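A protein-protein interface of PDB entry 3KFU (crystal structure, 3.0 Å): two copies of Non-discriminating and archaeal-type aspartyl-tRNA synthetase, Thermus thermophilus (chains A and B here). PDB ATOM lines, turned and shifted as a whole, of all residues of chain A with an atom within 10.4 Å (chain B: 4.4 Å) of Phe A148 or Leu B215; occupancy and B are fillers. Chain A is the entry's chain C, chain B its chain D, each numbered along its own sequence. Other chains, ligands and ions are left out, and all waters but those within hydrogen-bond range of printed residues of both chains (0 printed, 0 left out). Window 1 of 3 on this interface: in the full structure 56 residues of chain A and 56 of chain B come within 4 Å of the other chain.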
ATOM      1  N   ARG A 136     -12.984   9.180   3.520  1.00  0.00           N
ATOM      2  CA  ARG A 136     -11.882   9.075   2.574  1.00  0.00           C
ATOM      3  C   ARG A 136     -12.396   8.771   1.167  1.00  0.00           C
ATOM      4  O   ARG A 136     -11.957   9.384   0.191  1.00  0.00           O
ATOM      5  CB  ARG A 136     -10.891   8.000   3.014  1.00  0.00           C
ATOM      6  CG  ARG A 136     -10.234   8.238   4.356  1.00  0.00           C
ATOM      7  CD  ARG A 136      -9.119   7.231   4.570  1.00  0.00           C
ATOM      8  NE  ARG A 136      -8.462   7.355   5.868  1.00  0.00           N
ATOM      9  CZ  ARG A 136      -8.715   6.569   6.910  1.00  0.00           C
ATOM     10  NH1 ARG A 136      -9.614   5.602   6.803  1.00  0.00           N
ATOM     11  NH2 ARG A 136      -8.068   6.745   8.055  1.00  0.00           N
ATOM     12  N   ASP A 140     -11.359  11.048  -1.940  1.00  0.00           N
ATOM     13  CA  ASP A 140     -10.506  10.407  -2.941  1.00  0.00           C
ATOM     14  C   ASP A 140     -11.118  10.535  -4.335  1.00  0.00           C
ATOM     15  O   ASP A 140     -10.448  10.944  -5.282  1.00  0.00           O
ATOM     16  CB  ASP A 140     -10.263   8.933  -2.597  1.00  0.00           C
ATOM     17  CG  ASP A 140      -9.218   8.746  -1.505  1.00  0.00           C
ATOM     18  OD1 ASP A 140      -8.353   9.636  -1.341  1.00  0.00           O
ATOM     19  OD2 ASP A 140      -9.255   7.700  -0.818  1.00  0.00           O
ATOM     20  N   PHE A 144      -8.773  14.264  -3.892  1.00  0.00           N
ATOM     21  CA  PHE A 144      -8.022  14.639  -2.704  1.00  0.00           C
ATOM     22  C   PHE A 144      -6.890  13.663  -2.436  1.00  0.00           C
ATOM     23  O   PHE A 144      -7.022  12.460  -2.662  1.00  0.00           O
ATOM     24  CB  PHE A 144      -8.935  14.726  -1.485  1.00  0.00           C
ATOM     25  CG  PHE A 144      -9.663  16.026  -1.376  1.00  0.00           C
ATOM     26  CD1 PHE A 144     -10.827  16.243  -2.089  1.00  0.00           C
ATOM     27  CD2 PHE A 144      -9.181  17.035  -0.561  1.00  0.00           C
ATOM     28  CE1 PHE A 144     -11.499  17.441  -1.991  1.00  0.00           C
ATOM     29  CE2 PHE A 144      -9.848  18.236  -0.456  1.00  0.00           C
ATOM     30  CZ  PHE A 144     -11.009  18.438  -1.173  1.00  0.00           C
ATOM     31  N   THR A 145      -5.774  14.196  -1.960  1.00  0.00           N
ATOM     32  CA  THR A 145      -4.640  13.376  -1.571  1.00  0.00           C
ATOM     33  C   THR A 145      -4.543  13.342  -0.047  1.00  0.00           C
ATOM     34  O   THR A 145      -4.562  14.379   0.614  1.00  0.00           O
ATOM     35  CB  THR A 145      -3.331  13.921  -2.160  1.00  0.00           C
ATOM     36  OG1 THR A 145      -3.504  14.173  -3.559  1.00  0.00           O
ATOM     37  CG2 THR A 145      -2.197  12.932  -1.959  1.00  0.00           C
ATOM     38  N   GLU A 146      -4.461  12.140   0.506  1.00  0.00           N
ATOM     39  CA  GLU A 146      -4.307  11.969   1.939  1.00  0.00           C
ATOM     40  C   GLU A 146      -2.867  12.286   2.322  1.00  0.00           C
ATOM     41  O   GLU A 146      -1.931  11.814   1.683  1.00  0.00           O
ATOM     42  CB  GLU A 146      -4.658  10.534   2.326  1.00  0.00           C
ATOM     43  CG  GLU A 146      -4.691  10.263   3.814  1.00  0.00           C
ATOM     44  CD  GLU A 146      -5.136   8.847   4.128  1.00  0.00           C
ATOM     45  OE1 GLU A 146      -4.950   7.961   3.268  1.00  0.00           O
ATOM     46  OE2 GLU A 146      -5.681   8.618   5.230  1.00  0.00           O
ATOM     47  N   ILE A 147      -2.686  13.099   3.354  1.00  0.00           N
ATOM     48  CA  ILE A 147      -1.344  13.460   3.793  1.00  0.00           C
ATOM     49  C   ILE A 147      -1.068  12.990   5.214  1.00  0.00           C
ATOM     50  O   ILE A 147      -1.982  12.749   5.996  1.00  0.00           O
ATOM     51  CB  ILE A 147      -1.103  14.970   3.702  1.00  0.00           C
ATOM     52  CG1 ILE A 147      -2.139  15.721   4.541  1.00  0.00           C
ATOM     53  CG2 ILE A 147      -1.147  15.426   2.251  1.00  0.00           C
ATOM     54  CD1 ILE A 147      -1.988  17.231   4.493  1.00  0.00           C
ATOM     55  N   PHE A 148       0.209  12.854   5.541  1.00  0.00           N
ATOM     56  CA  PHE A 148       0.600  12.380   6.854  1.00  0.00           C
ATOM     57  C   PHE A 148       1.625  13.338   7.448  1.00  0.00           C
ATOM     58  O   PHE A 148       2.818  13.255   7.163  1.00  0.00           O
ATOM     59  CB  PHE A 148       1.151  10.956   6.754  1.00  0.00           C
ATOM     60  CG  PHE A 148       0.244  10.012   6.013  1.00  0.00           C
ATOM     61  CD1 PHE A 148       0.407   9.800   4.652  1.00  0.00           C
ATOM     62  CD2 PHE A 148      -0.778   9.349   6.670  1.00  0.00           C
ATOM     63  CE1 PHE A 148      -0.426   8.939   3.963  1.00  0.00           C
ATOM     64  CE2 PHE A 148      -1.615   8.486   5.987  1.00  0.00           C
ATOM     65  CZ  PHE A 148      -1.440   8.282   4.632  1.00  0.00           C
ATOM     66  N   THR A 149       1.137  14.259   8.270  1.00  0.00           N
ATOM     67  CA  THR A 149       1.963  15.321   8.824  1.00  0.00           C
ATOM     68  C   THR A 149       2.365  14.996  10.259  1.00  0.00           C
ATOM     69  O   THR A 149       1.911  13.997  10.818  1.00  0.00           O
ATOM     70  CB  THR A 149       1.218  16.673   8.783  1.00  0.00           C
ATOM     71  OG1 THR A 149       0.136  16.656   9.719  1.00  0.00           O
ATOM     72  CG2 THR A 149       0.672  16.940   7.387  1.00  0.00           C
ATOM     73  N   PRO A 150       3.235  15.830  10.855  1.00  0.00           N
ATOM     74  CA  PRO A 150       3.660  15.644  12.249  1.00  0.00           C
ATOM     75  C   PRO A 150       2.538  15.923  13.245  1.00  0.00           C
ATOM     76  O   PRO A 150       2.603  15.417  14.368  1.00  0.00           O
ATOM     77  CB  PRO A 150       4.771  16.686  12.417  1.00  0.00           C
ATOM     78  CG  PRO A 150       5.234  16.986  11.027  1.00  0.00           C
ATOM     79  CD  PRO A 150       4.010  16.888  10.183  1.00  0.00           C
ATOM     80  N   PRO A 179       0.628  22.275  12.743  1.00  0.00           N
ATOM     81  CA  PRO A 179      -0.502  21.441  12.316  1.00  0.00           C
ATOM     82  C   PRO A 179      -1.324  22.133  11.238  1.00  0.00           C
ATOM     83  O   PRO A 179      -1.482  21.593  10.144  1.00  0.00           O
ATOM     84  CB  PRO A 179      -1.328  21.295  13.594  1.00  0.00           C
ATOM     85  CG  PRO A 179      -0.339  21.457  14.696  1.00  0.00           C
ATOM     86  CD  PRO A 179       0.648  22.472  14.203  1.00  0.00           C
ATOM     87  N   TYR A 182       1.133  22.952   8.104  1.00  0.00           N
ATOM     88  CA  TYR A 182       1.497  21.849   7.225  1.00  0.00           C
ATOM     89  C   TYR A 182       0.421  21.542   6.180  1.00  0.00           C
ATOM     90  O   TYR A 182       0.727  21.388   5.000  1.00  0.00           O
ATOM     91  CB  TYR A 182       1.845  20.611   8.049  1.00  0.00           C
ATOM     92  CG  TYR A 182       3.067  20.807   8.923  1.00  0.00           C
ATOM     93  CD1 TYR A 182       4.155  21.544   8.470  1.00  0.00           C
ATOM     94  CD2 TYR A 182       3.128  20.269  10.202  1.00  0.00           C
ATOM     95  CE1 TYR A 182       5.271  21.730   9.261  1.00  0.00           C
ATOM     96  CE2 TYR A 182       4.242  20.451  11.000  1.00  0.00           C
ATOM     97  CZ  TYR A 182       5.309  21.183  10.525  1.00  0.00           C
ATOM     98  OH  TYR A 182       6.420  21.366  11.316  1.00  0.00           O
ATOM     99  N   LYS A 183      -0.835  21.460   6.608  1.00  0.00           N
ATOM    100  CA  LYS A 183      -1.939  21.312   5.664  1.00  0.00           C
ATOM    101  C   LYS A 183      -1.867  22.381   4.576  1.00  0.00           C
ATOM    102  O   LYS A 183      -1.901  22.073   3.388  1.00  0.00           O
ATOM    103  CB  LYS A 183      -3.283  21.385   6.384  1.00  0.00           C
ATOM    104  CG  LYS A 183      -3.524  20.230   7.335  1.00  0.00           C
ATOM    105  CD  LYS A 183      -4.591  20.564   8.372  1.00  0.00           C
ATOM    106  CE  LYS A 183      -4.766  19.416   9.356  1.00  0.00           C
ATOM    107  NZ  LYS A 183      -3.480  19.006   9.985  1.00  0.00           N
ATOM    108  N   MET A 186       0.822  22.015   2.117  1.00  0.00           N
ATOM    109  CA  MET A 186       0.496  20.906   1.225  1.00  0.00           C
ATOM    110  C   MET A 186      -0.530  21.268   0.152  1.00  0.00           C
ATOM    111  O   MET A 186      -0.693  20.540  -0.822  1.00  0.00           O
ATOM    112  CB  MET A 186      -0.004  19.711   2.034  1.00  0.00           C
ATOM    113  CG  MET A 186       1.060  19.076   2.901  1.00  0.00           C
ATOM    114  SD  MET A 186       2.472  18.527   1.931  1.00  0.00           S
ATOM    115  CE  MET A 186       1.705  17.304   0.864  1.00  0.00           C
ATOM    116  N   PHE A 190      -0.546  19.776  -3.565  1.00  0.00           N
ATOM    117  CA  PHE A 190      -1.532  18.847  -4.111  1.00  0.00           C
ATOM    118  C   PHE A 190      -2.880  19.506  -4.375  1.00  0.00           C
ATOM    119  O   PHE A 190      -3.797  18.864  -4.885  1.00  0.00           O
ATOM    120  CB  PHE A 190      -1.724  17.645  -3.180  1.00  0.00           C
ATOM    121  CG  PHE A 190      -0.562  16.686  -3.168  1.00  0.00           C
ATOM    122  CD1 PHE A 190      -0.111  16.140  -1.977  1.00  0.00           C
ATOM    123  CD2 PHE A 190       0.067  16.324  -4.345  1.00  0.00           C
ATOM    124  CE1 PHE A 190       0.951  15.259  -1.962  1.00  0.00           C
ATOM    125  CE2 PHE A 190       1.131  15.441  -4.336  1.00  0.00           C
ATOM    126  CZ  PHE A 190       1.574  14.908  -3.147  1.00  0.00           C
ATOM    127  N   VAL A 193      -6.168  18.340  -0.188  1.00  0.00           N
ATOM    128  CA  VAL A 193      -5.655  17.303   0.692  1.00  0.00           C
ATOM    129  C   VAL A 193      -6.571  17.087   1.885  1.00  0.00           C
ATOM    130  O   VAL A 193      -7.440  17.911   2.168  1.00  0.00           O
ATOM    131  CB  VAL A 193      -4.243  17.643   1.197  1.00  0.00           C
ATOM    132  CG1 VAL A 193      -3.294  17.821   0.029  1.00  0.00           C
ATOM    133  CG2 VAL A 193      -4.277  18.898   2.059  1.00  0.00           C
ATOM    134  N   TYR A 194      -6.379  15.964   2.569  1.00  0.00           N
ATOM    135  CA  TYR A 194      -7.102  15.678   3.799  1.00  0.00           C
ATOM    136  C   TYR A 194      -6.240  14.831   4.719  1.00  0.00           C
ATOM    137  O   TYR A 194      -5.217  14.297   4.302  1.00  0.00           O
ATOM    138  CB  TYR A 194      -8.428  14.974   3.515  1.00  0.00           C
ATOM    139  CG  TYR A 194      -8.292  13.544   3.045  1.00  0.00           C
ATOM    140  CD1 TYR A 194      -8.331  13.230   1.691  1.00  0.00           C
ATOM    141  CD2 TYR A 194      -8.134  12.507   3.952  1.00  0.00           C
ATOM    142  CE1 TYR A 194      -8.212  11.921   1.254  1.00  0.00           C
ATOM    143  CE2 TYR A 194      -8.011  11.196   3.523  1.00  0.00           C
ATOM    144  CZ  TYR A 194      -8.052  10.909   2.175  1.00  0.00           C
ATOM    145  OH  TYR A 194      -7.937   9.607   1.751  1.00  0.00           O
ATOM    146  N   GLU A 195      -6.645  14.723   5.976  1.00  0.00           N
ATOM    147  CA  GLU A 195      -5.891  13.940   6.942  1.00  0.00           C
ATOM    148  C   GLU A 195      -6.788  13.435   8.062  1.00  0.00           C
ATOM    149  O   GLU A 195      -7.741  14.102   8.464  1.00  0.00           O
ATOM    150  CB  GLU A 195      -4.737  14.760   7.517  1.00  0.00           C
ATOM    151  CG  GLU A 195      -3.779  13.950   8.370  1.00  0.00           C
ATOM    152  CD  GLU A 195      -2.518  14.716   8.719  1.00  0.00           C
ATOM    153  OE1 GLU A 195      -1.530  14.081   9.151  1.00  0.00           O
ATOM    154  OE2 GLU A 195      -2.514  15.953   8.559  1.00  0.00           O
ATOM    155  N   VAL A 196      -6.483  12.238   8.546  1.00  0.00           N
ATOM    156  CA  VAL A 196      -7.200  11.646   9.663  1.00  0.00           C
ATOM    157  C   VAL A 196      -6.183  11.374  10.752  1.00  0.00           C
ATOM    158  O   VAL A 196      -5.441  10.393  10.683  1.00  0.00           O
ATOM    159  CB  VAL A 196      -7.880  10.324   9.262  1.00  0.00           C
ATOM    160  CG1 VAL A 196      -8.439   9.616  10.482  1.00  0.00           C
ATOM    161  CG2 VAL A 196      -8.974  10.581   8.231  1.00  0.00           C
ATOM    162  N   ALA A 197      -6.137  12.252  11.746  1.00  0.00           N
ATOM    163  CA  ALA A 197      -5.111  12.169  12.775  1.00  0.00           C
ATOM    164  C   ALA A 197      -5.639  12.559  14.149  1.00  0.00           C
ATOM    165  O   ALA A 197      -6.634  13.275  14.256  1.00  0.00           O
ATOM    166  CB  ALA A 197      -3.925  13.040  12.397  1.00  0.00           C
ATOM    167  N   PRO A 198      -4.970  12.076  15.206  1.00  0.00           N
ATOM    168  CA  PRO A 198      -5.299  12.425  16.592  1.00  0.00           C
ATOM    169  C   PRO A 198      -4.867  13.850  16.909  1.00  0.00           C
ATOM    170  O   PRO A 198      -3.847  14.299  16.393  1.00  0.00           O
ATOM    171  CB  PRO A 198      -4.465  11.433  17.413  1.00  0.00           C
ATOM    172  CG  PRO A 198      -4.051  10.361  16.448  1.00  0.00           C
ATOM    173  CD  PRO A 198      -3.912  11.056  15.137  1.00  0.00           C
ATOM    174  N   ASP A 218      -9.576  16.280   8.906  1.00  0.00           N
ATOM    175  CA  ASP A 218      -9.235  17.599   8.385  1.00  0.00           C
ATOM    176  C   ASP A 218      -9.220  17.658   6.864  1.00  0.00           C
ATOM    177  O   ASP A 218      -8.591  16.834   6.207  1.00  0.00           O
ATOM    178  CB  ASP A 218      -7.879  18.053   8.931  1.00  0.00           C
ATOM    179  CG  ASP A 218      -7.832  18.062  10.447  1.00  0.00           C
ATOM    180  OD1 ASP A 218      -8.227  17.053  11.065  1.00  0.00           O
ATOM    181  OD2 ASP A 218      -7.401  19.083  11.024  1.00  0.00           O
ATOM    182  N   GLN B 128       2.802   6.967  -1.680  1.00  0.00           N
ATOM    183  CA  GLN B 128       2.605   6.451  -0.334  1.00  0.00           C
ATOM    184  C   GLN B 128       1.128   6.471   0.036  1.00  0.00           C
ATOM    185  O   GLN B 128       0.644   5.593   0.745  1.00  0.00           O
ATOM    186  CB  GLN B 128       3.405   7.263   0.676  1.00  0.00           C
ATOM    187  CG  GLN B 128       3.225   6.792   2.099  1.00  0.00           C
ATOM    188  CD  GLN B 128       4.116   7.532   3.062  1.00  0.00           C
ATOM    189  OE1 GLN B 128       3.702   8.514   3.676  1.00  0.00           O
ATOM    190  NE2 GLN B 128       5.354   7.068   3.197  1.00  0.00           N
ATOM    191  N   VAL B 132      -1.286   3.141   0.959  1.00  0.00           N
ATOM    192  CA  VAL B 132      -2.126   3.094   2.149  1.00  0.00           C
ATOM    193  C   VAL B 132      -3.600   2.884   1.797  1.00  0.00           C
ATOM    194  O   VAL B 132      -4.335   2.237   2.544  1.00  0.00           O
ATOM    195  CB  VAL B 132      -1.941   4.355   3.016  1.00  0.00           C
ATOM    196  CG1 VAL B 132      -2.891   4.337   4.198  1.00  0.00           C
ATOM    197  CG2 VAL B 132      -0.500   4.447   3.494  1.00  0.00           C
ATOM    198  N   VAL B 196      -3.565   2.963  11.035  1.00  0.00           N
ATOM    199  CA  VAL B 196      -2.551   3.745  10.343  1.00  0.00           C
ATOM    200  C   VAL B 196      -2.164   4.928  11.225  1.00  0.00           C
ATOM    201  O   VAL B 196      -2.819   5.970  11.199  1.00  0.00           O
ATOM    202  CB  VAL B 196      -3.072   4.272   8.999  1.00  0.00           C
ATOM    203  CG1 VAL B 196      -1.983   5.039   8.274  1.00  0.00           C
ATOM    204  CG2 VAL B 196      -3.568   3.127   8.150  1.00  0.00           C
ATOM    205  N   ALA B 197      -1.108   4.763  12.015  1.00  0.00           N
ATOM    206  CA  ALA B 197      -0.744   5.775  13.001  1.00  0.00           C
ATOM    207  C   ALA B 197       0.754   6.052  13.047  1.00  0.00           C
ATOM    208  O   ALA B 197       1.565   5.152  12.826  1.00  0.00           O
ATOM    209  CB  ALA B 197      -1.249   5.373  14.378  1.00  0.00           C
ATOM    210  N   PRO B 198       1.120   7.310  13.334  1.00  0.00           N
ATOM    211  CA  PRO B 198       2.509   7.759  13.486  1.00  0.00           C
ATOM    212  C   PRO B 198       3.153   7.192  14.746  1.00  0.00           C
ATOM    213  O   PRO B 198       2.470   7.012  15.750  1.00  0.00           O
ATOM    214  CB  PRO B 198       2.375   9.281  13.606  1.00  0.00           C
ATOM    215  CG  PRO B 198       1.031   9.599  13.032  1.00  0.00           C
ATOM    216  CD  PRO B 198       0.174   8.435  13.391  1.00  0.00           C
ATOM    217  N   TYR B 214       7.729   8.275  12.054  1.00  0.00           N
ATOM    218  CA  TYR B 214       7.331   7.593  10.828  1.00  0.00           C
ATOM    219  C   TYR B 214       5.900   7.067  10.891  1.00  0.00           C
ATOM    220  O   TYR B 214       5.330   6.914  11.969  1.00  0.00           O
ATOM    221  CB  TYR B 214       8.297   6.451  10.512  1.00  0.00           C
ATOM    222  CG  TYR B 214       8.188   5.265  11.441  1.00  0.00           C
ATOM    223  CD1 TYR B 214       7.446   4.145  11.086  1.00  0.00           C
ATOM    224  CD2 TYR B 214       8.833   5.261  12.670  1.00  0.00           C
ATOM    225  CE1 TYR B 214       7.348   3.054  11.930  1.00  0.00           C
ATOM    226  CE2 TYR B 214       8.738   4.175  13.523  1.00  0.00           C
ATOM    227  CZ  TYR B 214       7.996   3.074  13.147  1.00  0.00           C
ATOM    228  OH  TYR B 214       7.899   1.988  13.988  1.00  0.00           O
ATOM    229  N   LEU B 215       5.327   6.797   9.722  1.00  0.00           N
ATOM    230  CA  LEU B 215       3.982   6.242   9.635  1.00  0.00           C
ATOM    231  C   LEU B 215       4.026   4.719   9.699  1.00  0.00           C
ATOM    232  O   LEU B 215       4.783   4.081   8.968  1.00  0.00           O
ATOM    233  CB  LEU B 215       3.303   6.694   8.345  1.00  0.00           C
ATOM    234  CG  LEU B 215       1.856   6.230   8.179  1.00  0.00           C
ATOM    235  CD1 LEU B 215       1.022   6.723   9.341  1.00  0.00           C
ATOM    236  CD2 LEU B 215       1.278   6.711   6.860  1.00  0.00           C
ATOM    237  N   SER B 216       3.215   4.138  10.579  1.00  0.00           N
ATOM    238  CA  SER B 216       3.193   2.688  10.753  1.00  0.00           C
ATOM    239  C   SER B 216       1.828   2.080  10.441  1.00  0.00           C
ATOM    240  O   SER B 216       0.803   2.522  10.957  1.00  0.00           O
ATOM    241  CB  SER B 216       3.614   2.310  12.171  1.00  0.00           C
ATOM    242  OG  SER B 216       3.792   0.911  12.291  1.00  0.00           O
ATOM    243  N   LEU B 217       1.831   1.060   9.590  1.00  0.00           N
ATOM    244  CA  LEU B 217       0.619   0.329   9.254  1.00  0.00           C
ATOM    245  C   LEU B 217       0.601  -0.964  10.054  1.00  0.00           C
ATOM    246  O   LEU B 217       1.328  -1.907   9.744  1.00  0.00           O
ATOM    247  CB  LEU B 217       0.589   0.023   7.760  1.00  0.00           C
ATOM    248  CG  LEU B 217       1.030   1.187   6.877  1.00  0.00           C
ATOM    249  CD1 LEU B 217       1.001   0.785   5.409  1.00  0.00           C
ATOM    250  CD2 LEU B 217       0.161   2.409   7.129  1.00  0.00           C
ATOM    251  N   ILE B 392       3.971  -2.411   9.131  1.00  0.00           N
ATOM    252  CA  ILE B 392       4.744  -2.036   7.957  1.00  0.00           C
ATOM    253  C   ILE B 392       5.233  -0.602   8.085  1.00  0.00           C
ATOM    254  O   ILE B 392       4.479   0.284   8.482  1.00  0.00           O
ATOM    255  CB  ILE B 392       3.899  -2.149   6.678  1.00  0.00           C
ATOM    256  CG1 ILE B 392       3.255  -3.535   6.583  1.00  0.00           C
ATOM    257  CG2 ILE B 392       4.747  -1.854   5.454  1.00  0.00           C
ATOM    258  CD1 ILE B 392       2.235  -3.663   5.474  1.00  0.00           C
ATOM    259  N   GLY B 393       6.501  -0.378   7.753  1.00  0.00           N
ATOM    260  CA  GLY B 393       7.045   0.966   7.695  1.00  0.00           C
ATOM    261  C   GLY B 393       6.703   1.620   6.369  1.00  0.00           C
ATOM    262  O   GLY B 393       7.387   1.409   5.365  1.00  0.00           O
ATOM    263  N   ALA B 394       5.634   2.413   6.369  1.00  0.00           N
ATOM    264  CA  ALA B 394       5.147   3.069   5.162  1.00  0.00           C
ATOM    265  C   ALA B 394       6.249   3.757   4.345  1.00  0.00           C
ATOM    266  O   ALA B 394       6.368   3.535   3.137  1.00  0.00           O
ATOM    267  CB  ALA B 394       4.052   4.061   5.516  1.00  0.00           C
ATOM    268  N   GLU B 395       7.047   4.595   5.002  1.00  0.00           N
ATOM    269  CA  GLU B 395       8.090   5.341   4.304  1.00  0.00           C
ATOM    270  C   GLU B 395       9.180   4.431   3.751  1.00  0.00           C
ATOM    271  O   GLU B 395       9.653   4.635   2.637  1.00  0.00           O
ATOM    272  CB  GLU B 395       8.707   6.411   5.210  1.00  0.00           C
ATOM    273  CG  GLU B 395       7.777   7.563   5.553  1.00  0.00           C
ATOM    274  CD  GLU B 395       6.952   7.295   6.793  1.00  0.00           C
ATOM    275  OE1 GLU B 395       7.051   6.177   7.340  1.00  0.00           O
ATOM    276  OE2 GLU B 395       6.210   8.204   7.224  1.00  0.00           O
ATOM    277  N   ARG B 411       8.948  11.141   3.435  1.00  0.00           N
ATOM    278  CA  ARG B 411       8.238  11.895   4.459  1.00  0.00           C
ATOM    279  C   ARG B 411       8.024  13.328   3.995  1.00  0.00           C
ATOM    280  O   ARG B 411       8.923  13.941   3.425  1.00  0.00           O
ATOM    281  CB  ARG B 411       9.019  11.879   5.769  1.00  0.00           C
ATOM    282  CG  ARG B 411       8.233  12.387   6.958  1.00  0.00           C
ATOM    283  CD  ARG B 411       8.072  11.305   8.009  1.00  0.00           C
ATOM    284  NE  ARG B 411       6.668  11.003   8.277  1.00  0.00           N
ATOM    285  CZ  ARG B 411       5.901  11.696   9.111  1.00  0.00           C
ATOM    286  NH1 ARG B 411       6.397  12.741   9.758  1.00  0.00           N
ATOM    287  NH2 ARG B 411       4.635  11.348   9.293  1.00  0.00           N
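NE2 of Gln B128 sits close to N of Glu B395 (3.5 Å). O of Leu B215 is in hydrogen-bond range of N of Ala B394. OE2 of Glu B395 is in hydrogen-bond range of N of Leu B215 (3.0 Å). OE2 of Glu B395 lies within salt-bridge range of NE of Arg B411 (3.0 Å).
Phe A148 touches Gln B128. Leu B215 touches Phe A148 (CD2 to CD2, 3.3 Å).
Hydrophobic or aromatic side chains of chain A within 4 Å of the printed part of chain B: Phe A148. Among the printed residues, 3 pairs touch across the chains. Among the printed residues, no Asp or Glu carboxylate lies within 4 Å of a Lys or Arg side-chain nitrogen of the other chain.
Leu B215 touches just one residue of chain A: Phe A148. No residue of chain A comes within 4 Å of Val B196. No residue of chain A comes within 4 Å of Pro B198. No residue of chain A comes within 4 Å of Ser B216. Gly B393 touches none of the printed residues of chain A. No residue of chain A comes within 4 Å of Ala B394. Of the printed residues of chain A, Gln B128 touches Phe A148 (3.7 Å). Of the printed residues of chain A, Arg B411 touches Phe A148 (3.4 Å). Val B132 touches none of the printed residues of chain A. Asp A140 touches none of the printed residues of chain B. The nearest residue of chain B that does not touch Phe A148 is Val B132 (4.1 Å). The nearest printed residue of chain A that does not touch Arg B411 is Thr A149 (4.1 Å).
3 positions are printed for both chains. Of the 3 pairs that touch across the chains among the printed residues, none has its exchanged pair printed and touching as well.
The backbone carbonyl oxygen (O) of Phe A148 sits at hydrogen-bond distance from the guanidinium group (NH2) of Arg B411 (3.4 Å).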
